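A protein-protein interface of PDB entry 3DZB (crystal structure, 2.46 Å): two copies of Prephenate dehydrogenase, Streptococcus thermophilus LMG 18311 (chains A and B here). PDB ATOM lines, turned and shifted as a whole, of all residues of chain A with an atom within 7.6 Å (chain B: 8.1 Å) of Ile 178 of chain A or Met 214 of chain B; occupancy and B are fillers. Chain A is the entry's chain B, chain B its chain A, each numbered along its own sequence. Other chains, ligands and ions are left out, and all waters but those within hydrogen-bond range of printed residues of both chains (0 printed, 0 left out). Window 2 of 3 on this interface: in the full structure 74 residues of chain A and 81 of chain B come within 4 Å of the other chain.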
ATOM      1  N   LYS A 103     -24.488  22.306  21.551  1.00  0.00           N
ATOM      2  CA  LYS A 103     -25.136  23.180  20.575  1.00  0.00           C
ATOM      3  C   LYS A 103     -24.755  22.948  19.117  1.00  0.00           C
ATOM      4  O   LYS A 103     -25.619  22.715  18.285  1.00  0.00           O
ATOM      5  CB  LYS A 103     -24.815  24.629  20.947  1.00  0.00           C
ATOM      6  CG  LYS A 103     -25.987  25.512  21.347  1.00  0.00           C
ATOM      7  CD  LYS A 103     -26.840  24.917  22.427  1.00  0.00           C
ATOM      8  CE  LYS A 103     -27.890  24.007  21.819  1.00  0.00           C
ATOM      9  NZ  LYS A 103     -28.307  22.990  22.818  1.00  0.00           N
ATOM     10  N   VAL A 122     -33.191  28.905  16.430  1.00  0.00           N
ATOM     11  CA  VAL A 122     -32.036  29.401  17.165  1.00  0.00           C
ATOM     12  C   VAL A 122     -31.723  28.296  18.168  1.00  0.00           C
ATOM     13  O   VAL A 122     -32.623  27.567  18.595  1.00  0.00           O
ATOM     14  CB  VAL A 122     -32.356  30.722  17.940  1.00  0.00           C
ATOM     15  CG1 VAL A 122     -33.328  30.439  19.081  1.00  0.00           C
ATOM     16  CG2 VAL A 122     -31.062  31.352  18.467  1.00  0.00           C
ATOM     17  N   GLY A 123     -30.455  28.159  18.534  1.00  0.00           N
ATOM     18  CA  GLY A 123     -30.093  27.133  19.498  1.00  0.00           C
ATOM     19  C   GLY A 123     -30.405  27.554  20.921  1.00  0.00           C
ATOM     20  O   GLY A 123     -30.407  28.741  21.248  1.00  0.00           O
ATOM     21  N   TYR A 147     -28.083  30.608  33.657  1.00  0.00           N
ATOM     22  CA  TYR A 147     -28.036  31.061  32.279  1.00  0.00           C
ATOM     23  C   TYR A 147     -28.978  30.287  31.340  1.00  0.00           C
ATOM     24  O   TYR A 147     -29.169  29.075  31.467  1.00  0.00           O
ATOM     25  CB  TYR A 147     -26.616  30.955  31.737  1.00  0.00           C
ATOM     26  CG  TYR A 147     -25.680  32.039  32.204  1.00  0.00           C
ATOM     27  CD1 TYR A 147     -25.969  33.384  31.964  1.00  0.00           C
ATOM     28  CD2 TYR A 147     -24.497  31.729  32.869  1.00  0.00           C
ATOM     29  CE1 TYR A 147     -25.104  34.393  32.379  1.00  0.00           C
ATOM     30  CE2 TYR A 147     -23.619  32.734  33.287  1.00  0.00           C
ATOM     31  CZ  TYR A 147     -23.931  34.064  33.040  1.00  0.00           C
ATOM     32  OH  TYR A 147     -23.089  35.066  33.468  1.00  0.00           O
ATOM     33  N   ILE A 149     -28.968  29.990  27.543  1.00  0.00           N
ATOM     34  CA  ILE A 149     -28.114  30.334  26.420  1.00  0.00           C
ATOM     35  C   ILE A 149     -28.706  30.158  25.023  1.00  0.00           C
ATOM     36  O   ILE A 149     -29.226  29.093  24.669  1.00  0.00           O
ATOM     37  CB  ILE A 149     -26.806  29.535  26.511  1.00  0.00           C
ATOM     38  CG1 ILE A 149     -26.316  29.533  27.962  1.00  0.00           C
ATOM     39  CG2 ILE A 149     -25.749  30.153  25.615  1.00  0.00           C
ATOM     40  CD1 ILE A 149     -25.129  28.617  28.218  1.00  0.00           C
ATOM     41  N   PHE A 150     -28.614  31.229  24.239  1.00  0.00           N
ATOM     42  CA  PHE A 150     -29.086  31.255  22.859  1.00  0.00           C
ATOM     43  C   PHE A 150     -27.878  31.138  21.943  1.00  0.00           C
ATOM     44  O   PHE A 150     -26.857  31.790  22.176  1.00  0.00           O
ATOM     45  CB  PHE A 150     -29.748  32.597  22.516  1.00  0.00           C
ATOM     46  CG  PHE A 150     -31.033  32.868  23.236  1.00  0.00           C
ATOM     47  CD1 PHE A 150     -32.201  32.208  22.878  1.00  0.00           C
ATOM     48  CD2 PHE A 150     -31.083  33.822  24.242  1.00  0.00           C
ATOM     49  CE1 PHE A 150     -33.403  32.499  23.506  1.00  0.00           C
ATOM     50  CE2 PHE A 150     -32.280  34.122  24.877  1.00  0.00           C
ATOM     51  CZ  PHE A 150     -33.445  33.458  24.509  1.00  0.00           C
ATOM     52  N   THR A 151     -27.982  30.316  20.907  1.00  0.00           N
ATOM     53  CA  THR A 151     -26.895  30.218  19.942  1.00  0.00           C
ATOM     54  C   THR A 151     -27.491  30.541  18.580  1.00  0.00           C
ATOM     55  O   THR A 151     -28.303  29.779  18.045  1.00  0.00           O
ATOM     56  CB  THR A 151     -26.224  28.819  19.919  1.00  0.00           C
ATOM     57  OG1 THR A 151     -27.199  27.803  19.651  1.00  0.00           O
ATOM     58  CG2 THR A 151     -25.527  28.550  21.262  1.00  0.00           C
ATOM     59  N   PRO A 152     -27.125  31.705  18.016  1.00  0.00           N
ATOM     60  CA  PRO A 152     -27.642  32.115  16.705  1.00  0.00           C
ATOM     61  C   PRO A 152     -27.352  31.104  15.599  1.00  0.00           C
ATOM     62  O   PRO A 152     -26.278  30.488  15.562  1.00  0.00           O
ATOM     63  CB  PRO A 152     -26.940  33.455  16.460  1.00  0.00           C
ATOM     64  CG  PRO A 152     -26.780  34.009  17.852  1.00  0.00           C
ATOM     65  CD  PRO A 152     -26.318  32.783  18.622  1.00  0.00           C
ATOM     66  N   THR A 153     -28.327  30.932  14.708  1.00  0.00           N
ATOM     67  CA  THR A 153     -28.189  30.016  13.580  1.00  0.00           C
ATOM     68  C   THR A 153     -28.592  30.774  12.319  1.00  0.00           C
ATOM     69  O   THR A 153     -29.325  31.756  12.384  1.00  0.00           O
ATOM     70  CB  THR A 153     -29.115  28.788  13.720  1.00  0.00           C
ATOM     71  OG1 THR A 153     -30.409  29.096  13.192  1.00  0.00           O
ATOM     72  CG2 THR A 153     -29.267  28.398  15.188  1.00  0.00           C
ATOM     73  N   ILE A 161     -35.044  35.750  18.801  1.00  0.00           N
ATOM     74  CA  ILE A 161     -34.626  35.788  20.205  1.00  0.00           C
ATOM     75  C   ILE A 161     -35.449  36.739  21.078  1.00  0.00           C
ATOM     76  O   ILE A 161     -35.849  36.387  22.191  1.00  0.00           O
ATOM     77  CB  ILE A 161     -33.133  36.165  20.329  1.00  0.00           C
ATOM     78  CG1 ILE A 161     -32.275  35.126  19.597  1.00  0.00           C
ATOM     79  CG2 ILE A 161     -32.745  36.261  21.806  1.00  0.00           C
ATOM     80  CD1 ILE A 161     -30.809  35.440  19.593  1.00  0.00           C
ATOM     81  N   VAL A 176     -28.227  35.121  27.522  1.00  0.00           N
ATOM     82  CA  VAL A 176     -26.908  35.301  26.960  1.00  0.00           C
ATOM     83  C   VAL A 176     -26.898  34.589  25.615  1.00  0.00           C
ATOM     84  O   VAL A 176     -27.592  33.594  25.424  1.00  0.00           O
ATOM     85  CB  VAL A 176     -25.810  34.720  27.875  1.00  0.00           C
ATOM     86  CG1 VAL A 176     -26.159  33.300  28.276  1.00  0.00           C
ATOM     87  CG2 VAL A 176     -24.471  34.745  27.152  1.00  0.00           C
ATOM     88  N   GLU A 177     -26.123  35.126  24.683  1.00  0.00           N
ATOM     89  CA  GLU A 177     -26.019  34.578  23.348  1.00  0.00           C
ATOM     90  C   GLU A 177     -24.563  34.316  23.085  1.00  0.00           C
ATOM     91  O   GLU A 177     -23.700  35.112  23.453  1.00  0.00           O
ATOM     92  CB  GLU A 177     -26.532  35.580  22.313  1.00  0.00           C
ATOM     93  CG  GLU A 177     -27.997  35.949  22.455  1.00  0.00           C
ATOM     94  CD  GLU A 177     -28.342  37.231  21.716  1.00  0.00           C
ATOM     95  OE1 GLU A 177     -27.867  37.406  20.567  1.00  0.00           O
ATOM     96  OE2 GLU A 177     -29.089  38.053  22.293  1.00  0.00           O
ATOM     97  N   ILE A 178     -24.285  33.198  22.445  1.00  0.00           N
ATOM     98  CA  ILE A 178     -22.912  32.864  22.138  1.00  0.00           C
ATOM     99  C   ILE A 178     -22.883  31.980  20.901  1.00  0.00           C
ATOM    100  O   ILE A 178     -23.878  31.354  20.550  1.00  0.00           O
ATOM    101  CB  ILE A 178     -22.239  32.126  23.334  1.00  0.00           C
ATOM    102  CG1 ILE A 178     -20.740  31.964  23.067  1.00  0.00           C
ATOM    103  CG2 ILE A 178     -22.891  30.754  23.554  1.00  0.00           C
ATOM    104  CD1 ILE A 178     -19.977  31.305  24.200  1.00  0.00           C
ATOM    105  N   ASP A 179     -21.749  31.951  20.223  1.00  0.00           N
ATOM    106  CA  ASP A 179     -21.628  31.100  19.060  1.00  0.00           C
ATOM    107  C   ASP A 179     -21.798  29.659  19.547  1.00  0.00           C
ATOM    108  O   ASP A 179     -21.344  29.313  20.641  1.00  0.00           O
ATOM    109  CB  ASP A 179     -20.256  31.275  18.420  1.00  0.00           C
ATOM    110  CG  ASP A 179     -20.028  30.301  17.309  1.00  0.00           C
ATOM    111  OD1 ASP A 179     -19.166  29.411  17.464  1.00  0.00           O
ATOM    112  OD2 ASP A 179     -20.728  30.421  16.282  1.00  0.00           O
ATOM    113  N   ALA A 180     -22.460  28.829  18.746  1.00  0.00           N
ATOM    114  CA  ALA A 180     -22.681  27.435  19.105  1.00  0.00           C
ATOM    115  C   ALA A 180     -21.365  26.708  19.395  1.00  0.00           C
ATOM    116  O   ALA A 180     -21.211  26.094  20.448  1.00  0.00           O
ATOM    117  CB  ALA A 180     -23.429  26.729  17.992  1.00  0.00           C
ATOM    118  N   ALA A 181     -20.426  26.788  18.454  1.00  0.00           N
ATOM    119  CA  ALA A 181     -19.124  26.148  18.592  1.00  0.00           C
ATOM    120  C   ALA A 181     -18.438  26.557  19.898  1.00  0.00           C
ATOM    121  O   ALA A 181     -17.928  25.709  20.626  1.00  0.00           O
ATOM    122  CB  ALA A 181     -18.248  26.497  17.391  1.00  0.00           C
ATOM    123  N   GLU A 182     -18.421  27.854  20.193  1.00  0.00           N
ATOM    124  CA  GLU A 182     -17.814  28.348  21.431  1.00  0.00           C
ATOM    125  C   GLU A 182     -18.496  27.744  22.662  1.00  0.00           C
ATOM    126  O   GLU A 182     -17.836  27.347  23.628  1.00  0.00           O
ATOM    127  CB  GLU A 182     -17.925  29.863  21.505  1.00  0.00           C
ATOM    128  CG  GLU A 182     -16.646  30.575  21.182  1.00  0.00           C
ATOM    129  CD  GLU A 182     -15.587  30.337  22.214  1.00  0.00           C
ATOM    130  OE1 GLU A 182     -15.708  30.878  23.331  1.00  0.00           O
ATOM    131  OE2 GLU A 182     -14.631  29.602  21.905  1.00  0.00           O
ATOM    132  N   HIS A 183     -19.822  27.701  22.628  1.00  0.00           N
ATOM    133  CA  HIS A 183     -20.591  27.131  23.719  1.00  0.00           C
ATOM    134  C   HIS A 183     -20.049  25.742  24.020  1.00  0.00           C
ATOM    135  O   HIS A 183     -19.792  25.393  25.174  1.00  0.00           O
ATOM    136  CB  HIS A 183     -22.069  27.043  23.326  1.00  0.00           C
ATOM    137  CG  HIS A 183     -22.885  26.180  24.236  1.00  0.00           C
ATOM    138  ND1 HIS A 183     -22.873  24.806  24.164  1.00  0.00           N
ATOM    139  CD2 HIS A 183     -23.705  26.497  25.263  1.00  0.00           C
ATOM    140  CE1 HIS A 183     -23.648  24.312  25.113  1.00  0.00           C
ATOM    141  NE2 HIS A 183     -24.163  25.317  25.797  1.00  0.00           N
ATOM    142  N   ASP A 184     -19.868  24.958  22.964  1.00  0.00           N
ATOM    143  CA  ASP A 184     -19.360  23.603  23.090  1.00  0.00           C
ATOM    144  C   ASP A 184     -17.963  23.548  23.689  1.00  0.00           C
ATOM    145  O   ASP A 184     -17.673  22.667  24.493  1.00  0.00           O
ATOM    146  CB  ASP A 184     -19.385  22.918  21.729  1.00  0.00           C
ATOM    147  CG  ASP A 184     -20.789  22.559  21.291  1.00  0.00           C
ATOM    148  OD1 ASP A 184     -21.765  22.854  22.025  1.00  0.00           O
ATOM    149  OD2 ASP A 184     -20.917  21.970  20.204  1.00  0.00           O
ATOM    150  N   ARG A 185     -17.104  24.489  23.297  1.00  0.00           N
ATOM    151  CA  ARG A 185     -15.744  24.545  23.823  1.00  0.00           C
ATOM    152  C   ARG A 185     -15.774  24.900  25.298  1.00  0.00           C
ATOM    153  O   ARG A 185     -15.087  24.279  26.113  1.00  0.00           O
ATOM    154  CB  ARG A 185     -14.911  25.601  23.106  1.00  0.00           C
ATOM    155  CG  ARG A 185     -14.644  25.339  21.642  1.00  0.00           C
ATOM    156  CD  ARG A 185     -13.688  26.381  21.078  1.00  0.00           C
ATOM    157  NE  ARG A 185     -13.751  26.410  19.623  1.00  0.00           N
ATOM    158  CZ  ARG A 185     -14.505  27.250  18.921  1.00  0.00           C
ATOM    159  NH1 ARG A 185     -15.261  28.147  19.542  1.00  0.00           N
ATOM    160  NH2 ARG A 185     -14.515  27.179  17.598  1.00  0.00           N
ATOM    161  N   VAL A 186     -16.575  25.906  25.635  1.00  0.00           N
ATOM    162  CA  VAL A 186     -16.686  26.361  27.013  1.00  0.00           C
ATOM    163  C   VAL A 186     -17.300  25.315  27.930  1.00  0.00           C
ATOM    164  O   VAL A 186     -16.776  25.052  29.007  1.00  0.00           O
ATOM    165  CB  VAL A 186     -17.533  27.649  27.128  1.00  0.00           C
ATOM    166  CG1 VAL A 186     -17.540  28.125  28.568  1.00  0.00           C
ATOM    167  CG2 VAL A 186     -16.974  28.734  26.230  1.00  0.00           C
ATOM    168  N   THR A 187     -18.418  24.728  27.512  1.00  0.00           N
ATOM    169  CA  THR A 187     -19.069  23.719  28.336  1.00  0.00           C
ATOM    170  C   THR A 187     -18.213  22.458  28.440  1.00  0.00           C
ATOM    171  O   THR A 187     -18.290  21.720  29.419  1.00  0.00           O
ATOM    172  CB  THR A 187     -20.496  23.403  27.821  1.00  0.00           C
ATOM    173  OG1 THR A 187     -20.467  23.044  26.432  1.00  0.00           O
ATOM    174  CG2 THR A 187     -21.385  24.620  28.020  1.00  0.00           C
ATOM    175  N   ILE A 190     -15.565  23.414  31.432  1.00  0.00           N
ATOM    176  CA  ILE A 190     -16.055  23.504  32.803  1.00  0.00           C
ATOM    177  C   ILE A 190     -17.198  22.572  33.196  1.00  0.00           C
ATOM    178  O   ILE A 190     -17.694  22.646  34.314  1.00  0.00           O
ATOM    179  CB  ILE A 190     -16.456  24.969  33.157  1.00  0.00           C
ATOM    180  CG1 ILE A 190     -17.329  25.578  32.050  1.00  0.00           C
ATOM    181  CG2 ILE A 190     -15.206  25.814  33.388  1.00  0.00           C
ATOM    182  CD1 ILE A 190     -18.767  25.104  32.055  1.00  0.00           C
ATOM    183  N   TYR B 208      -7.451  28.236  29.946  1.00  0.00           N
ATOM    184  CA  TYR B 208      -8.465  28.194  28.910  1.00  0.00           C
ATOM    185  C   TYR B 208      -9.340  29.452  28.898  1.00  0.00           C
ATOM    186  O   TYR B 208      -9.776  29.900  27.840  1.00  0.00           O
ATOM    187  CB  TYR B 208      -9.321  26.942  29.086  1.00  0.00           C
ATOM    188  CG  TYR B 208     -10.002  26.488  27.820  1.00  0.00           C
ATOM    189  CD1 TYR B 208     -11.381  26.539  27.699  1.00  0.00           C
ATOM    190  CD2 TYR B 208      -9.262  26.001  26.748  1.00  0.00           C
ATOM    191  CE1 TYR B 208     -12.015  26.114  26.544  1.00  0.00           C
ATOM    192  CE2 TYR B 208      -9.884  25.572  25.584  1.00  0.00           C
ATOM    193  CZ  TYR B 208     -11.264  25.636  25.489  1.00  0.00           C
ATOM    194  OH  TYR B 208     -11.900  25.258  24.336  1.00  0.00           O
ATOM    195  N   ALA B 209      -9.591  30.030  30.066  1.00  0.00           N
ATOM    196  CA  ALA B 209     -10.396  31.242  30.145  1.00  0.00           C
ATOM    197  C   ALA B 209      -9.735  32.392  29.379  1.00  0.00           C
ATOM    198  O   ALA B 209     -10.408  33.253  28.825  1.00  0.00           O
ATOM    199  CB  ALA B 209     -10.593  31.639  31.592  1.00  0.00           C
ATOM    200  N   GLN B 210      -8.413  32.408  29.347  1.00  0.00           N
ATOM    201  CA  GLN B 210      -7.704  33.475  28.649  1.00  0.00           C
ATOM    202  C   GLN B 210      -8.164  33.638  27.205  1.00  0.00           C
ATOM    203  O   GLN B 210      -8.236  34.759  26.694  1.00  0.00           O
ATOM    204  CB  GLN B 210      -6.190  33.221  28.686  1.00  0.00           C
ATOM    205  CG  GLN B 210      -5.608  33.278  30.084  1.00  0.00           C
ATOM    206  CD  GLN B 210      -4.155  32.880  30.124  1.00  0.00           C
ATOM    207  OE1 GLN B 210      -3.792  31.763  29.750  1.00  0.00           O
ATOM    208  NE2 GLN B 210      -3.306  33.794  30.577  1.00  0.00           N
ATOM    209  N   ALA B 211      -8.477  32.527  26.546  1.00  0.00           N
ATOM    210  CA  ALA B 211      -8.901  32.590  25.154  1.00  0.00           C
ATOM    211  C   ALA B 211     -10.378  32.327  24.989  1.00  0.00           C
ATOM    212  O   ALA B 211     -10.879  32.310  23.868  1.00  0.00           O
ATOM    213  CB  ALA B 211      -8.104  31.600  24.310  1.00  0.00           C
ATOM    214  N   HIS B 212     -11.071  32.109  26.103  1.00  0.00           N
ATOM    215  CA  HIS B 212     -12.509  31.847  26.082  1.00  0.00           C
ATOM    216  C   HIS B 212     -13.074  32.462  27.351  1.00  0.00           C
ATOM    217  O   HIS B 212     -13.185  31.783  28.367  1.00  0.00           O
ATOM    218  CB  HIS B 212     -12.760  30.345  26.074  1.00  0.00           C
ATOM    219  CG  HIS B 212     -12.029  29.622  24.991  1.00  0.00           C
ATOM    220  ND1 HIS B 212     -12.415  29.674  23.668  1.00  0.00           N
ATOM    221  CD2 HIS B 212     -10.906  28.866  25.024  1.00  0.00           C
ATOM    222  CE1 HIS B 212     -11.562  28.980  22.935  1.00  0.00           C
ATOM    223  NE2 HIS B 212     -10.636  28.480  23.733  1.00  0.00           N
ATOM    224  N   GLU B 213     -13.447  33.738  27.286  1.00  0.00           N
ATOM    225  CA  GLU B 213     -13.942  34.454  28.457  1.00  0.00           C
ATOM    226  C   GLU B 213     -15.147  33.884  29.195  1.00  0.00           C
ATOM    227  O   GLU B 213     -15.260  34.051  30.407  1.00  0.00           O
ATOM    228  CB  GLU B 213     -14.203  35.933  28.110  1.00  0.00           C
ATOM    229  CG  GLU B 213     -15.421  36.258  27.211  1.00  0.00           C
ATOM    230  CD  GLU B 213     -15.232  35.883  25.745  1.00  0.00           C
ATOM    231  OE1 GLU B 213     -14.108  36.059  25.213  1.00  0.00           O
ATOM    232  OE2 GLU B 213     -16.219  35.426  25.115  1.00  0.00           O
ATOM    233  N   MET B 214     -16.043  33.205  28.492  1.00  0.00           N
ATOM    234  CA  MET B 214     -17.229  32.657  29.143  1.00  0.00           C
ATOM    235  C   MET B 214     -16.924  31.497  30.082  1.00  0.00           C
ATOM    236  O   MET B 214     -17.779  31.086  30.875  1.00  0.00           O
ATOM    237  CB  MET B 214     -18.252  32.230  28.092  1.00  0.00           C
ATOM    238  CG  MET B 214     -18.767  33.394  27.256  1.00  0.00           C
ATOM    239  SD  MET B 214     -19.330  34.891  28.367  1.00  0.00           S
ATOM    240  CE  MET B 214     -20.896  34.098  29.180  1.00  0.00           C
ATOM    241  N   THR B 215     -15.701  30.977  29.984  1.00  0.00           N
ATOM    242  CA  THR B 215     -15.252  29.880  30.827  1.00  0.00           C
ATOM    243  C   THR B 215     -15.523  30.182  32.302  1.00  0.00           C
ATOM    244  O   THR B 215     -16.042  29.341  33.028  1.00  0.00           O
ATOM    245  CB  THR B 215     -13.748  29.626  30.618  1.00  0.00           C
ATOM    246  OG1 THR B 215     -13.545  29.153  29.287  1.00  0.00           O
ATOM    247  CG2 THR B 215     -13.207  28.600  31.602  1.00  0.00           C
ATOM    248  N   ASN B 216     -15.196  31.388  32.743  1.00  0.00           N
ATOM    249  CA  ASN B 216     -15.409  31.740  34.143  1.00  0.00           C
ATOM    250  C   ASN B 216     -16.879  31.916  34.511  1.00  0.00           C
ATOM    251  O   ASN B 216     -17.269  31.668  35.650  1.00  0.00           O
ATOM    252  CB  ASN B 216     -14.659  33.027  34.494  1.00  0.00           C
ATOM    253  CG  ASN B 216     -13.364  33.170  33.730  1.00  0.00           C
ATOM    254  OD1 ASN B 216     -13.294  33.894  32.721  1.00  0.00           O
ATOM    255  ND2 ASN B 216     -12.325  32.471  34.195  1.00  0.00           N
ATOM    256  N   HIS B 217     -17.696  32.330  33.552  1.00  0.00           N
ATOM    257  CA  HIS B 217     -19.109  32.565  33.829  1.00  0.00           C
ATOM    258  C   HIS B 217     -19.996  31.339  33.843  1.00  0.00           C
ATOM    259  O   HIS B 217     -20.834  31.192  34.736  1.00  0.00           O
ATOM    260  CB  HIS B 217     -19.640  33.589  32.844  1.00  0.00           C
ATOM    261  CG  HIS B 217     -18.903  34.882  32.901  1.00  0.00           C
ATOM    262  ND1 HIS B 217     -18.934  35.698  34.010  1.00  0.00           N
ATOM    263  CD2 HIS B 217     -18.054  35.465  32.025  1.00  0.00           C
ATOM    264  CE1 HIS B 217     -18.132  36.730  33.815  1.00  0.00           C
ATOM    265  NE2 HIS B 217     -17.585  36.612  32.618  1.00  0.00           N
ATOM    266  N   PHE B 218     -19.816  30.467  32.857  1.00  0.00           N
ATOM    267  CA  PHE B 218     -20.602  29.245  32.764  1.00  0.00           C
ATOM    268  C   PHE B 218     -20.224  28.219  33.830  1.00  0.00           C
ATOM    269  O   PHE B 218     -20.958  27.273  34.059  1.00  0.00           O
ATOM    270  CB  PHE B 218     -20.450  28.625  31.371  1.00  0.00           C
ATOM    271  CG  PHE B 218     -21.165  29.384  30.280  1.00  0.00           C
ATOM    272  CD1 PHE B 218     -21.914  30.521  30.568  1.00  0.00           C
ATOM    273  CD2 PHE B 218     -21.095  28.957  28.963  1.00  0.00           C
ATOM    274  CE1 PHE B 218     -22.576  31.216  29.560  1.00  0.00           C
ATOM    275  CE2 PHE B 218     -21.751  29.643  27.953  1.00  0.00           C
ATOM    276  CZ  PHE B 218     -22.493  30.775  28.252  1.00  0.00           C
ATOM    277  N   ALA B 219     -19.083  28.411  34.484  1.00  0.00           N
ATOM    278  CA  ALA B 219     -18.636  27.491  35.522  1.00  0.00           C
ATOM    279  C   ALA B 219     -19.717  27.426  36.592  1.00  0.00           C
ATOM    280  O   ALA B 219     -20.184  28.463  37.069  1.00  0.00           O
ATOM    281  CB  ALA B 219     -17.316  27.979  36.123  1.00  0.00           C
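The side-chain carboxylate of Glu 182 of chain A is in hydrogen-bond range of a ring nitrogen (ND1) of His 212 of chain B, at 2.8 Å.
The backbone carbonyl oxygen (O) of His 212 of chain B lies within hydrogen-bond range of the side-chain hydroxyl (OG1) of Thr 215 of chain B. The backbone NH (N) of Ile 178 of chain A lies within hydrogen-bond range of the backbone carbonyl oxygen (O) of Phe 150 of chain A (2.9 Å). OD1 of Asp 179 of chain A lies within hydrogen-bond range of N of Glu 182 of chain A, at 3.2 Å. The side-chain carboxylate of Glu 182 of chain A lies within salt-bridge range of the guanidinium group of Arg 185 of chain A (2.8 Å).
CD2 of Tyr 147 of chain A touches CD1 of Phe 218 of chain B, at 3.7 Å. CZ of Phe 218 of chain B touches CD1 of Ile 149 of chain A, at 3.4 Å. CD1 of Ile 178 of chain A touches CG of Met 214 of chain B (3.9 Å). Tyr 208 of chain B touches Arg 185 of chain A. CE1 of His 212 of chain B touches CD of Arg 185 of chain A, at 3.8 Å. Val 186 of chain A touches Met 214 of chain B. Thr 215 of chain B touches Val 186 of chain A. Phe 218 of chain B touches Val 186 of chain A (CD2 to CG1, 3.7 Å). Ile 190 of chain A touches Thr 215 of chain B (CG2 to O, 3.6 Å). Ile 190 of chain A touches Phe 218 of chain B.
Printed residues of chain B within 4 Å of Ile 149 of chain A: Phe 218 (3.4 Å). Printed residues of chain B within 4 Å of Glu 182 of chain A: His 212 (2.8 Å). Printed residues of chain B within 4 Å of Arg 185 of chain A: Tyr 208 and His 212. Met 214 of chain B touches just these residues of chain A: Ile 178 and Val 186. Printed residues of chain A within 4 Å of Thr 215 of chain B: Val 186 and Ile 190. Printed residues of chain A within 4 Å of His 217 of chain B: Tyr 147. The nearest residue of chain B that does not touch Ile 178 of chain A is Phe 218 of chain B (4.5 Å). The nearest residue of chain A that does not touch Met 214 of chain B is Val 176 of chain A (4.2 Å). The nearest printed residue of chain A that does not touch Phe 218 of chain B is Val 176 of chain A (4.3 Å).
Printed residues of chain A that touch a printed residue of chain B: Tyr 147, Ile 149, Ile 178, Glu 182, Arg 185, Val 186 and Ile 190. Hydrophobic or aromatic side chains of chain A that line the printed part of chain B: Tyr 147, Ile 149, Ile 178, Val 186 and Ile 190. Among the printed residues, 12 pairs touch across the chains. Among the printed residues, no Asp or Glu carboxylate lies within 4 Å of a Lys or Arg side-chain nitrogen of the other chain.
No position is printed for both chains. Of the 12 pairs that touch across the chains among the printed residues, none has its exchanged pair printed and touching as well.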
